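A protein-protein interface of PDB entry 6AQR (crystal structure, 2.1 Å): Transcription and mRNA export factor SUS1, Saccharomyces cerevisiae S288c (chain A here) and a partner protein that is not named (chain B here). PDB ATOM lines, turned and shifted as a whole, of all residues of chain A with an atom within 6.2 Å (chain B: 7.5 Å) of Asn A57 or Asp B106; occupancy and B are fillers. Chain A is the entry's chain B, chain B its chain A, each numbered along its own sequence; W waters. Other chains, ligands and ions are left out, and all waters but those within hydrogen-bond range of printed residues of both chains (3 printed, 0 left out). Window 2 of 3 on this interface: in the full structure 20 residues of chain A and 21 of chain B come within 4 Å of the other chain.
The backbone carbonyl oxygen of Glu B105 sits at hydrogen-bond distance from the side-chain hydroxyl of Thr A59 (2.7 Å).
The side-chain carboxylate (OD1) of Asp B106 sits at hydrogen-bond distance from the backbone NH (N) of Phe A58.
Asn A57 touches two residues of chain B.
Printed residues of chain A within 4 Å of Asp B106: Thr A56 (3.99 Å), Asn A57 (3.7 Å) and Phe A58 (2.8 Å).
Of the printed residues of chain A, Glu B105 touches Asn A57 (3.95 Å) and Thr A59 (2.7 Å).
Of the printed residues of chain A, Tyr B107 touches Phe A58 (3.7 Å).
Printed residues of chain B within 4 Å of Phe A58: Trp B74, Phe B100, Asp B106 and Tyr B107.
Gly B109 touches none of the printed residues of chain A.
Phe B102 touches none of the printed residues of chain A.
The nearest residue of chain B that does not touch Asn A57 is Cys B104 (4.3 Å).
The nearest printed residue of chain A that does not touch Asp B106 is Thr A59 (4.9 Å).
The nearest printed residue of chain A that does not touch Tyr B107 is Asn A57 (6.4 Å).
N of Cys B101 is in hydrogen-bond range of O of Asp B106 (2.9 Å).
The side-chain hydroxyl (OG) of Ser A55 sits at hydrogen-bond distance from the backbone NH (N) of Asn A57, at 3.2 Å.
The side-chain amide oxygen (OD1) of Asn A57 lies within hydrogen-bond range of the backbone NH (N) of Thr A59.
OD1 of Asn A57 sits at hydrogen-bond distance from N of Gln A60, 3.1 Å away.
Of the 17 printed residues of chain B, 5 touch a printed residue of chain A.
Printed residues of chain B that touch a printed residue of chain A: Trp B74, Phe B100, Glu B105, Asp B106 and Tyr B107.
Printed residues of chain A that touch a printed residue of chain B: Thr A56, Asn A57, Phe A58, Thr A59 and Leu A62.
Hydrophobic or aromatic side chains of chain A that line the printed part of chain B: Phe A58 and Leu A62.
Among the printed residues, 10 pairs touch across the chains.
OD1 of Asp B106 touches O of Thr A56, at 3.99 Å.
Asn A57 touches Glu B105 (OD1 to O, 3.95 Å).
Asn A57 touches Asp B106 (CA to OD2, 3.7 Å).
CH2 of Trp B74 touches CE1 of Phe A58, at 3.96 Å.
Phe A58 touches Phe B100 (CD1 to CE1, 3.8 Å).
CG of Phe A58 touches CE1 of Tyr B107 (3.7 Å).
Thr A59 touches Trp B74.
CD2 of Leu A62 touches NE1 of Trp B74, 3.6 Å away.
Water W1 bridges the side-chain hydroxyl of Thr A56 and the side-chain carboxylate of Asp B106.
Water W2 lies within hydrogen-bond range of OG1 of Thr A59 (2.7 Å) and OE2 of Glu B105 (3.1 Å).
Water W3 bridges OD1 of Asp B106 and O of Thr A56.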
ATOM      1  N   ASN A  53      23.128  10.273 -36.922  1.00  0.00           N
ATOM      2  CA  ASN A  53      24.282  10.007 -36.070  1.00  0.00           C
ATOM      3  C   ASN A  53      25.345   9.058 -36.674  1.00  0.00           C
ATOM      4  O   ASN A  53      26.478   9.013 -36.173  1.00  0.00           O
ATOM      5  CB  ASN A  53      23.826   9.466 -34.699  1.00  0.00           C
ATOM      6  CG  ASN A  53      24.915   9.553 -33.647  1.00  0.00           C
ATOM      7  OD1 ASN A  53      25.325   8.545 -33.006  1.00  0.00           O
ATOM      8  ND2 ASN A  53      25.419  10.754 -33.475  1.00  0.00           N
ATOM      9  N   SER A  55      25.593   5.885 -36.321  1.00  0.00           N
ATOM     10  CA  SER A  55      26.033   5.081 -35.189  1.00  0.00           C
ATOM     11  C   SER A  55      24.782   4.725 -34.388  1.00  0.00           C
ATOM     12  O   SER A  55      23.861   5.541 -34.289  1.00  0.00           O
ATOM     13  CB  SER A  55      26.996   5.856 -34.294  1.00  0.00           C
ATOM     14  OG  SER A  55      27.271   5.123 -33.100  1.00  0.00           O
ATOM     15  N   THR A  56      24.788   3.540 -33.813  1.00  0.00           N
ATOM     16  CA  THR A  56      23.679   3.060 -32.992  1.00  0.00           C
ATOM     17  C   THR A  56      23.964   3.195 -31.529  1.00  0.00           C
ATOM     18  O   THR A  56      23.213   2.650 -30.734  1.00  0.00           O
ATOM     19  CB  THR A  56      23.351   1.579 -33.299  1.00  0.00           C
ATOM     20  OG1 THR A  56      24.497   0.800 -33.019  1.00  0.00           O
ATOM     21  CG2 THR A  56      23.016   1.400 -34.757  1.00  0.00           C
ATOM     22  N   ASN A  57      25.046   3.906 -31.164  1.00  0.00           N
ATOM     23  CA  ASN A  57      25.413   4.085 -29.749  1.00  0.00           C
ATOM     24  C   ASN A  57      24.246   4.629 -28.888  1.00  0.00           C
ATOM     25  O   ASN A  57      23.751   5.748 -29.094  1.00  0.00           O
ATOM     26  CB  ASN A  57      26.579   5.010 -29.622  1.00  0.00           C
ATOM     27  CG  ASN A  57      26.993   5.219 -28.169  1.00  0.00           C
ATOM     28  OD1 ASN A  57      26.371   5.962 -27.417  1.00  0.00           O
ATOM     29  ND2 ASN A  57      28.069   4.546 -27.775  1.00  0.00           N
ATOM     30  N   PHE A  58      23.813   3.826 -27.906  1.00  0.00           N
ATOM     31  CA  PHE A  58      22.582   4.143 -27.182  1.00  0.00           C
ATOM     32  C   PHE A  58      22.671   5.496 -26.462  1.00  0.00           C
ATOM     33  O   PHE A  58      21.697   6.247 -26.429  1.00  0.00           O
ATOM     34  CB  PHE A  58      22.240   3.044 -26.189  1.00  0.00           C
ATOM     35  CG  PHE A  58      21.049   3.386 -25.316  1.00  0.00           C
ATOM     36  CD1 PHE A  58      21.213   3.892 -24.041  1.00  0.00           C
ATOM     37  CD2 PHE A  58      19.728   3.163 -25.811  1.00  0.00           C
ATOM     38  CE1 PHE A  58      20.096   4.175 -23.262  1.00  0.00           C
ATOM     39  CE2 PHE A  58      18.624   3.461 -25.051  1.00  0.00           C
ATOM     40  CZ  PHE A  58      18.796   3.957 -23.782  1.00  0.00           C
ATOM     41  N   THR A  59      23.822   5.818 -25.856  1.00  0.00           N
ATOM     42  CA  THR A  59      23.918   7.087 -25.114  1.00  0.00           C
ATOM     43  C   THR A  59      23.717   8.314 -26.011  1.00  0.00           C
ATOM     44  O   THR A  59      22.954   9.247 -25.683  1.00  0.00           O
ATOM     45  CB  THR A  59      25.261   7.171 -24.366  1.00  0.00           C
ATOM     46  OG1 THR A  59      25.283   6.132 -23.367  1.00  0.00           O
ATOM     47  CG2 THR A  59      25.384   8.530 -23.696  1.00  0.00           C
ATOM     48  N   GLN A  60      24.388   8.281 -27.165  1.00  0.00           N
ATOM     49  CA  GLN A  60      24.274   9.363 -28.129  1.00  0.00           C
ATOM     50  C   GLN A  60      22.829   9.431 -28.633  1.00  0.00           C
ATOM     51  O   GLN A  60      22.217  10.493 -28.611  1.00  0.00           O
ATOM     52  CB  GLN A  60      25.237   9.144 -29.300  1.00  0.00           C
ATOM     53  CG  GLN A  60      26.720   9.233 -28.903  1.00  0.00           C
ATOM     54  CD  GLN A  60      27.670   8.486 -29.857  1.00  0.00           C
ATOM     55  OE1 GLN A  60      28.648   7.840 -29.399  1.00  0.00           O
ATOM     56  NE2 GLN A  60      27.395   8.555 -31.184  1.00  0.00           N
ATOM     57  N   ILE A  61      22.293   8.304 -29.104  1.00  0.00           N
ATOM     58  CA  ILE A  61      20.905   8.325 -29.688  1.00  0.00           C
ATOM     59  C   ILE A  61      19.876   8.812 -28.666  1.00  0.00           C
ATOM     60  O   ILE A  61      19.053   9.623 -29.020  1.00  0.00           O
ATOM     61  CB  ILE A  61      20.530   6.937 -30.217  1.00  0.00           C
ATOM     62  CG1 ILE A  61      21.567   6.513 -31.296  1.00  0.00           C
ATOM     63  CG2 ILE A  61      19.064   6.899 -30.704  1.00  0.00           C
ATOM     64  CD1 ILE A  61      21.694   7.525 -32.433  1.00  0.00           C
ATOM     65  N   LEU A  62      19.949   8.303 -27.414  1.00  0.00           N
ATOM     66  CA  LEU A  62      19.000   8.675 -26.342  1.00  0.00           C
ATOM     67  C   LEU A  62      19.055  10.173 -26.012  1.00  0.00           C
ATOM     68  O   LEU A  62      17.998  10.855 -25.919  1.00  0.00           O
ATOM     69  CB  LEU A  62      19.237   7.834 -25.078  1.00  0.00           C
ATOM     70  CG  LEU A  62      18.264   8.248 -23.959  1.00  0.00           C
ATOM     71  CD1 LEU A  62      16.856   7.745 -24.322  1.00  0.00           C
ATOM     72  CD2 LEU A  62      18.753   7.702 -22.636  1.00  0.00           C
ATOM     73  N   SER B   7      34.089  -3.512 -33.450  1.00  0.00           N
ATOM     74  CA  SER B   7      32.626  -3.270 -33.457  1.00  0.00           C
ATOM     75  C   SER B   7      31.895  -4.046 -32.332  1.00  0.00           C
ATOM     76  O   SER B   7      30.719  -3.877 -32.151  1.00  0.00           O
ATOM     77  CB  SER B   7      32.036  -3.553 -34.852  1.00  0.00           C
ATOM     78  OG  SER B   7      32.145  -4.915 -35.185  1.00  0.00           O
ATOM     79  N   CYS B   9      31.756  -4.884 -28.034  1.00  0.00           N
ATOM     80  CA  CYS B   9      32.263  -4.428 -26.739  1.00  0.00           C
ATOM     81  C   CYS B   9      33.496  -5.267 -26.412  1.00  0.00           C
ATOM     82  O   CYS B   9      33.412  -6.485 -26.462  1.00  0.00           O
ATOM     83  CB  CYS B   9      31.181  -4.566 -25.693  1.00  0.00           C
ATOM     84  SG  CYS B   9      31.810  -4.664 -24.011  1.00  0.00           S
ATOM     85  N   TRP B  74      19.008   4.622 -14.224  1.00  0.00           N
ATOM     86  CA  TRP B  74      19.598   5.416 -15.273  1.00  0.00           C
ATOM     87  C   TRP B  74      19.573   6.911 -14.895  1.00  0.00           C
ATOM     88  O   TRP B  74      20.593   7.569 -14.986  1.00  0.00           O
ATOM     89  CB  TRP B  74      18.848   5.233 -16.603  1.00  0.00           C
ATOM     90  CG  TRP B  74      19.449   6.033 -17.725  1.00  0.00           C
ATOM     91  CD1 TRP B  74      19.061   7.282 -18.154  1.00  0.00           C
ATOM     92  CD2 TRP B  74      20.585   5.643 -18.562  1.00  0.00           C
ATOM     93  NE1 TRP B  74      19.851   7.673 -19.219  1.00  0.00           N
ATOM     94  CE2 TRP B  74      20.779   6.685 -19.502  1.00  0.00           C
ATOM     95  CE3 TRP B  74      21.424   4.517 -18.606  1.00  0.00           C
ATOM     96  CZ2 TRP B  74      21.776   6.627 -20.491  1.00  0.00           C
ATOM     97  CZ3 TRP B  74      22.432   4.436 -19.592  1.00  0.00           C
ATOM     98  CH2 TRP B  74      22.615   5.509 -20.519  1.00  0.00           C
ATOM     99  N   ILE B  89      30.595  -3.758 -14.213  1.00  0.00           N
ATOM    100  CA  ILE B  89      30.319  -2.875 -15.360  1.00  0.00           C
ATOM    101  C   ILE B  89      29.124  -3.330 -16.278  1.00  0.00           C
ATOM    102  O   ILE B  89      28.803  -2.645 -17.227  1.00  0.00           O
ATOM    103  CB  ILE B  89      31.621  -2.635 -16.161  1.00  0.00           C
ATOM    104  CG1 ILE B  89      32.057  -3.922 -16.871  1.00  0.00           C
ATOM    105  CG2 ILE B  89      32.738  -2.128 -15.219  1.00  0.00           C
ATOM    106  CD1 ILE B  89      33.066  -3.714 -17.997  1.00  0.00           C
ATOM    107  N   PHE B  90      28.562  -4.515 -16.023  1.00  0.00           N
ATOM    108  CA  PHE B  90      27.463  -5.110 -16.833  1.00  0.00           C
ATOM    109  C   PHE B  90      26.156  -5.159 -16.063  1.00  0.00           C
ATOM    110  O   PHE B  90      26.111  -5.683 -14.903  1.00  0.00           O
ATOM    111  CB  PHE B  90      27.821  -6.505 -17.329  1.00  0.00           C
ATOM    112  CG  PHE B  90      29.073  -6.538 -18.177  1.00  0.00           C
ATOM    113  CD1 PHE B  90      29.155  -5.809 -19.394  1.00  0.00           C
ATOM    114  CD2 PHE B  90      30.183  -7.314 -17.775  1.00  0.00           C
ATOM    115  CE1 PHE B  90      30.311  -5.864 -20.185  1.00  0.00           C
ATOM    116  CE2 PHE B  90      31.364  -7.351 -18.568  1.00  0.00           C
ATOM    117  CZ  PHE B  90      31.427  -6.614 -19.760  1.00  0.00           C
ATOM    118  N   LEU B  99      21.475  -6.349 -22.312  1.00  0.00           N
ATOM    119  CA  LEU B  99      22.767  -6.257 -21.599  1.00  0.00           C
ATOM    120  C   LEU B  99      23.514  -4.968 -21.990  1.00  0.00           C
ATOM    121  O   LEU B  99      23.753  -4.732 -23.160  1.00  0.00           O
ATOM    122  CB  LEU B  99      23.616  -7.492 -21.956  1.00  0.00           C
ATOM    123  CG  LEU B  99      24.970  -7.563 -21.225  1.00  0.00           C
ATOM    124  CD1 LEU B  99      24.769  -7.705 -19.693  1.00  0.00           C
ATOM    125  CD2 LEU B  99      25.768  -8.709 -21.808  1.00  0.00           C
ATOM    126  N   PHE B 100      23.762  -4.103 -20.991  1.00  0.00           N
ATOM    127  CA  PHE B 100      24.441  -2.824 -21.140  1.00  0.00           C
ATOM    128  C   PHE B 100      25.855  -2.928 -20.527  1.00  0.00           C
ATOM    129  O   PHE B 100      26.043  -3.497 -19.411  1.00  0.00           O
ATOM    130  CB  PHE B 100      23.704  -1.734 -20.357  1.00  0.00           C
ATOM    131  CG  PHE B 100      24.016  -0.310 -20.821  1.00  0.00           C
ATOM    132  CD1 PHE B 100      23.384   0.256 -21.916  1.00  0.00           C
ATOM    133  CD2 PHE B 100      24.930   0.491 -20.107  1.00  0.00           C
ATOM    134  CE1 PHE B 100      23.647   1.581 -22.297  1.00  0.00           C
ATOM    135  CE2 PHE B 100      25.165   1.780 -20.456  1.00  0.00           C
ATOM    136  CZ  PHE B 100      24.564   2.341 -21.592  1.00  0.00           C
ATOM    137  N   CYS B 101      26.810  -2.364 -21.252  1.00  0.00           N
ATOM    138  CA  CYS B 101      28.185  -2.206 -20.792  1.00  0.00           C
ATOM    139  C   CYS B 101      28.358  -0.744 -20.318  1.00  0.00           C
ATOM    140  O   CYS B 101      28.312   0.210 -21.116  1.00  0.00           O
ATOM    141  CB  CYS B 101      29.185  -2.556 -21.917  1.00  0.00           C
ATOM    142  SG  CYS B 101      30.878  -2.202 -21.281  1.00  0.00           S
ATOM    143  N   PHE B 102      28.548  -0.562 -19.032  1.00  0.00           N
ATOM    144  CA  PHE B 102      28.736   0.779 -18.487  1.00  0.00           C
ATOM    145  C   PHE B 102      30.100   1.441 -18.748  1.00  0.00           C
ATOM    146  O   PHE B 102      30.213   2.648 -18.557  1.00  0.00           O
ATOM    147  CB  PHE B 102      28.311   0.830 -17.015  1.00  0.00           C
ATOM    148  CG  PHE B 102      26.811   0.841 -16.869  1.00  0.00           C
ATOM    149  CD1 PHE B 102      26.061  -0.362 -16.833  1.00  0.00           C
ATOM    150  CD2 PHE B 102      26.143   2.049 -16.869  1.00  0.00           C
ATOM    151  CE1 PHE B 102      24.667  -0.308 -16.741  1.00  0.00           C
ATOM    152  CE2 PHE B 102      24.760   2.107 -16.780  1.00  0.00           C
ATOM    153  CZ  PHE B 102      24.020   0.952 -16.705  1.00  0.00           C
ATOM    154  N   LYS B 103      31.095   0.659 -19.188  1.00  0.00           N
ATOM    155  CA  LYS B 103      32.357   1.213 -19.706  1.00  0.00           C
ATOM    156  C   LYS B 103      32.211   1.725 -21.131  1.00  0.00           C
ATOM    157  O   LYS B 103      32.576   2.867 -21.395  1.00  0.00           O
ATOM    158  CB  LYS B 103      33.507   0.205 -19.572  1.00  0.00           C
ATOM    159  CG  LYS B 103      34.113   0.172 -18.158  1.00  0.00           C
ATOM    160  CD  LYS B 103      35.580  -0.301 -18.072  1.00  0.00           C
ATOM    161  CE  LYS B 103      36.630   0.637 -18.682  1.00  0.00           C
ATOM    162  NZ  LYS B 103      36.727   1.973 -18.008  1.00  0.00           N
ATOM    163  N   CYS B 104      31.673   0.912 -22.053  1.00  0.00           N
ATOM    164  CA  CYS B 104      31.286   1.418 -23.417  1.00  0.00           C
ATOM    165  C   CYS B 104      30.185   2.507 -23.357  1.00  0.00           C
ATOM    166  O   CYS B 104      30.114   3.377 -24.204  1.00  0.00           O
ATOM    167  CB  CYS B 104      30.793   0.288 -24.334  1.00  0.00           C
ATOM    168  SG  CYS B 104      32.002  -0.991 -24.704  1.00  0.00           S
ATOM    169  N   GLU B 105      29.338   2.465 -22.338  1.00  0.00           N
ATOM    170  CA  GLU B 105      28.092   3.295 -22.318  1.00  0.00           C
ATOM    171  C   GLU B 105      27.158   2.925 -23.503  1.00  0.00           C
ATOM    172  O   GLU B 105      26.508   3.788 -24.118  1.00  0.00           O
ATOM    173  CB  GLU B 105      28.380   4.807 -22.224  1.00  0.00           C
ATOM    174  CG  GLU B 105      29.001   5.216 -20.888  1.00  0.00           C
ATOM    175  CD  GLU B 105      29.163   6.735 -20.745  1.00  0.00           C
ATOM    176  OE1 GLU B 105      29.673   7.412 -21.682  1.00  0.00           O
ATOM    177  OE2 GLU B 105      28.790   7.266 -19.679  1.00  0.00           O
ATOM    178  N   ASP B 106      27.100   1.632 -23.802  1.00  0.00           N
ATOM    179  CA  ASP B 106      26.245   1.125 -24.892  1.00  0.00           C
ATOM    180  C   ASP B 106      25.714  -0.244 -24.536  1.00  0.00           C
ATOM    181  O   ASP B 106      26.338  -1.011 -23.757  1.00  0.00           O
ATOM    182  CB  ASP B 106      27.028   1.077 -26.242  1.00  0.00           C
ATOM    183  CG  ASP B 106      26.095   1.047 -27.507  1.00  0.00           C
ATOM    184  OD1 ASP B 106      24.863   1.251 -27.381  1.00  0.00           O
ATOM    185  OD2 ASP B 106      26.609   0.795 -28.635  1.00  0.00           O
ATOM    186  N   TYR B 107      24.594  -0.610 -25.153  1.00  0.00           N
ATOM    187  CA  TYR B 107      24.139  -1.991 -25.063  1.00  0.00           C
ATOM    188  C   TYR B 107      24.978  -2.915 -25.877  1.00  0.00           C
ATOM    189  O   TYR B 107      25.506  -2.534 -26.953  1.00  0.00           O
ATOM    190  CB  TYR B 107      22.703  -2.083 -25.571  1.00  0.00           C
ATOM    191  CG  TYR B 107      21.715  -1.597 -24.571  1.00  0.00           C
ATOM    192  CD1 TYR B 107      21.153  -0.313 -24.688  1.00  0.00           C
ATOM    193  CD2 TYR B 107      21.313  -2.427 -23.467  1.00  0.00           C
ATOM    194  CE1 TYR B 107      20.238   0.149 -23.735  1.00  0.00           C
ATOM    195  CE2 TYR B 107      20.366  -1.946 -22.513  1.00  0.00           C
ATOM    196  CZ  TYR B 107      19.849  -0.675 -22.647  1.00  0.00           C
ATOM    197  OH  TYR B 107      18.912  -0.177 -21.711  1.00  0.00           O
ATOM    198  N   ILE B 108      25.126  -4.148 -25.367  1.00  0.00           N
ATOM    199  CA  ILE B 108      25.732  -5.215 -26.168  1.00  0.00           C
ATOM    200  C   ILE B 108      24.588  -5.924 -26.970  1.00  0.00           C
ATOM    201  O   ILE B 108      23.933  -6.793 -26.430  1.00  0.00           O
ATOM    202  CB  ILE B 108      26.509  -6.194 -25.267  1.00  0.00           C
ATOM    203  CG1 ILE B 108      27.609  -5.407 -24.516  1.00  0.00           C
ATOM    204  CG2 ILE B 108      27.094  -7.338 -26.136  1.00  0.00           C
ATOM    205  CD1 ILE B 108      28.003  -5.991 -23.182  1.00  0.00           C
ATOM    206  N   GLY B 109      24.317  -5.526 -28.218  1.00  0.00           N
ATOM    207  CA  GLY B 109      23.207  -6.177 -28.967  1.00  0.00           C
ATOM    208  C   GLY B 109      23.607  -7.038 -30.150  1.00  0.00           C
ATOM    209  O   GLY B 109      22.745  -7.566 -30.869  1.00  0.00           O
ATOM    210  N   ASN B 110      24.920  -7.176 -30.401  1.00  0.00           N
ATOM    211  CA  ASN B 110      25.360  -7.781 -31.640  1.00  0.00           C
ATOM    212  C   ASN B 110      26.173  -9.087 -31.456  1.00  0.00           C
ATOM    213  O   ASN B 110      26.977  -9.461 -32.323  1.00  0.00           O
ATOM    214  CB  ASN B 110      26.115  -6.747 -32.462  1.00  0.00           C
ATOM    215  CG  ASN B 110      27.327  -6.191 -31.735  1.00  0.00           C
ATOM    216  OD1 ASN B 110      27.594  -6.546 -30.576  1.00  0.00           O
ATOM    217  ND2 ASN B 110      28.038  -5.292 -32.399  1.00  0.00           N
HETATM  218  O   HOH W   1      26.028   0.250 -31.154  1.00  0.00           O
HETATM  219  O   HOH W   2      25.934   6.594 -20.744  1.00  0.00           O
HETATM  220  O   HOH W   3      22.499   0.240 -28.723  1.00  0.00           O
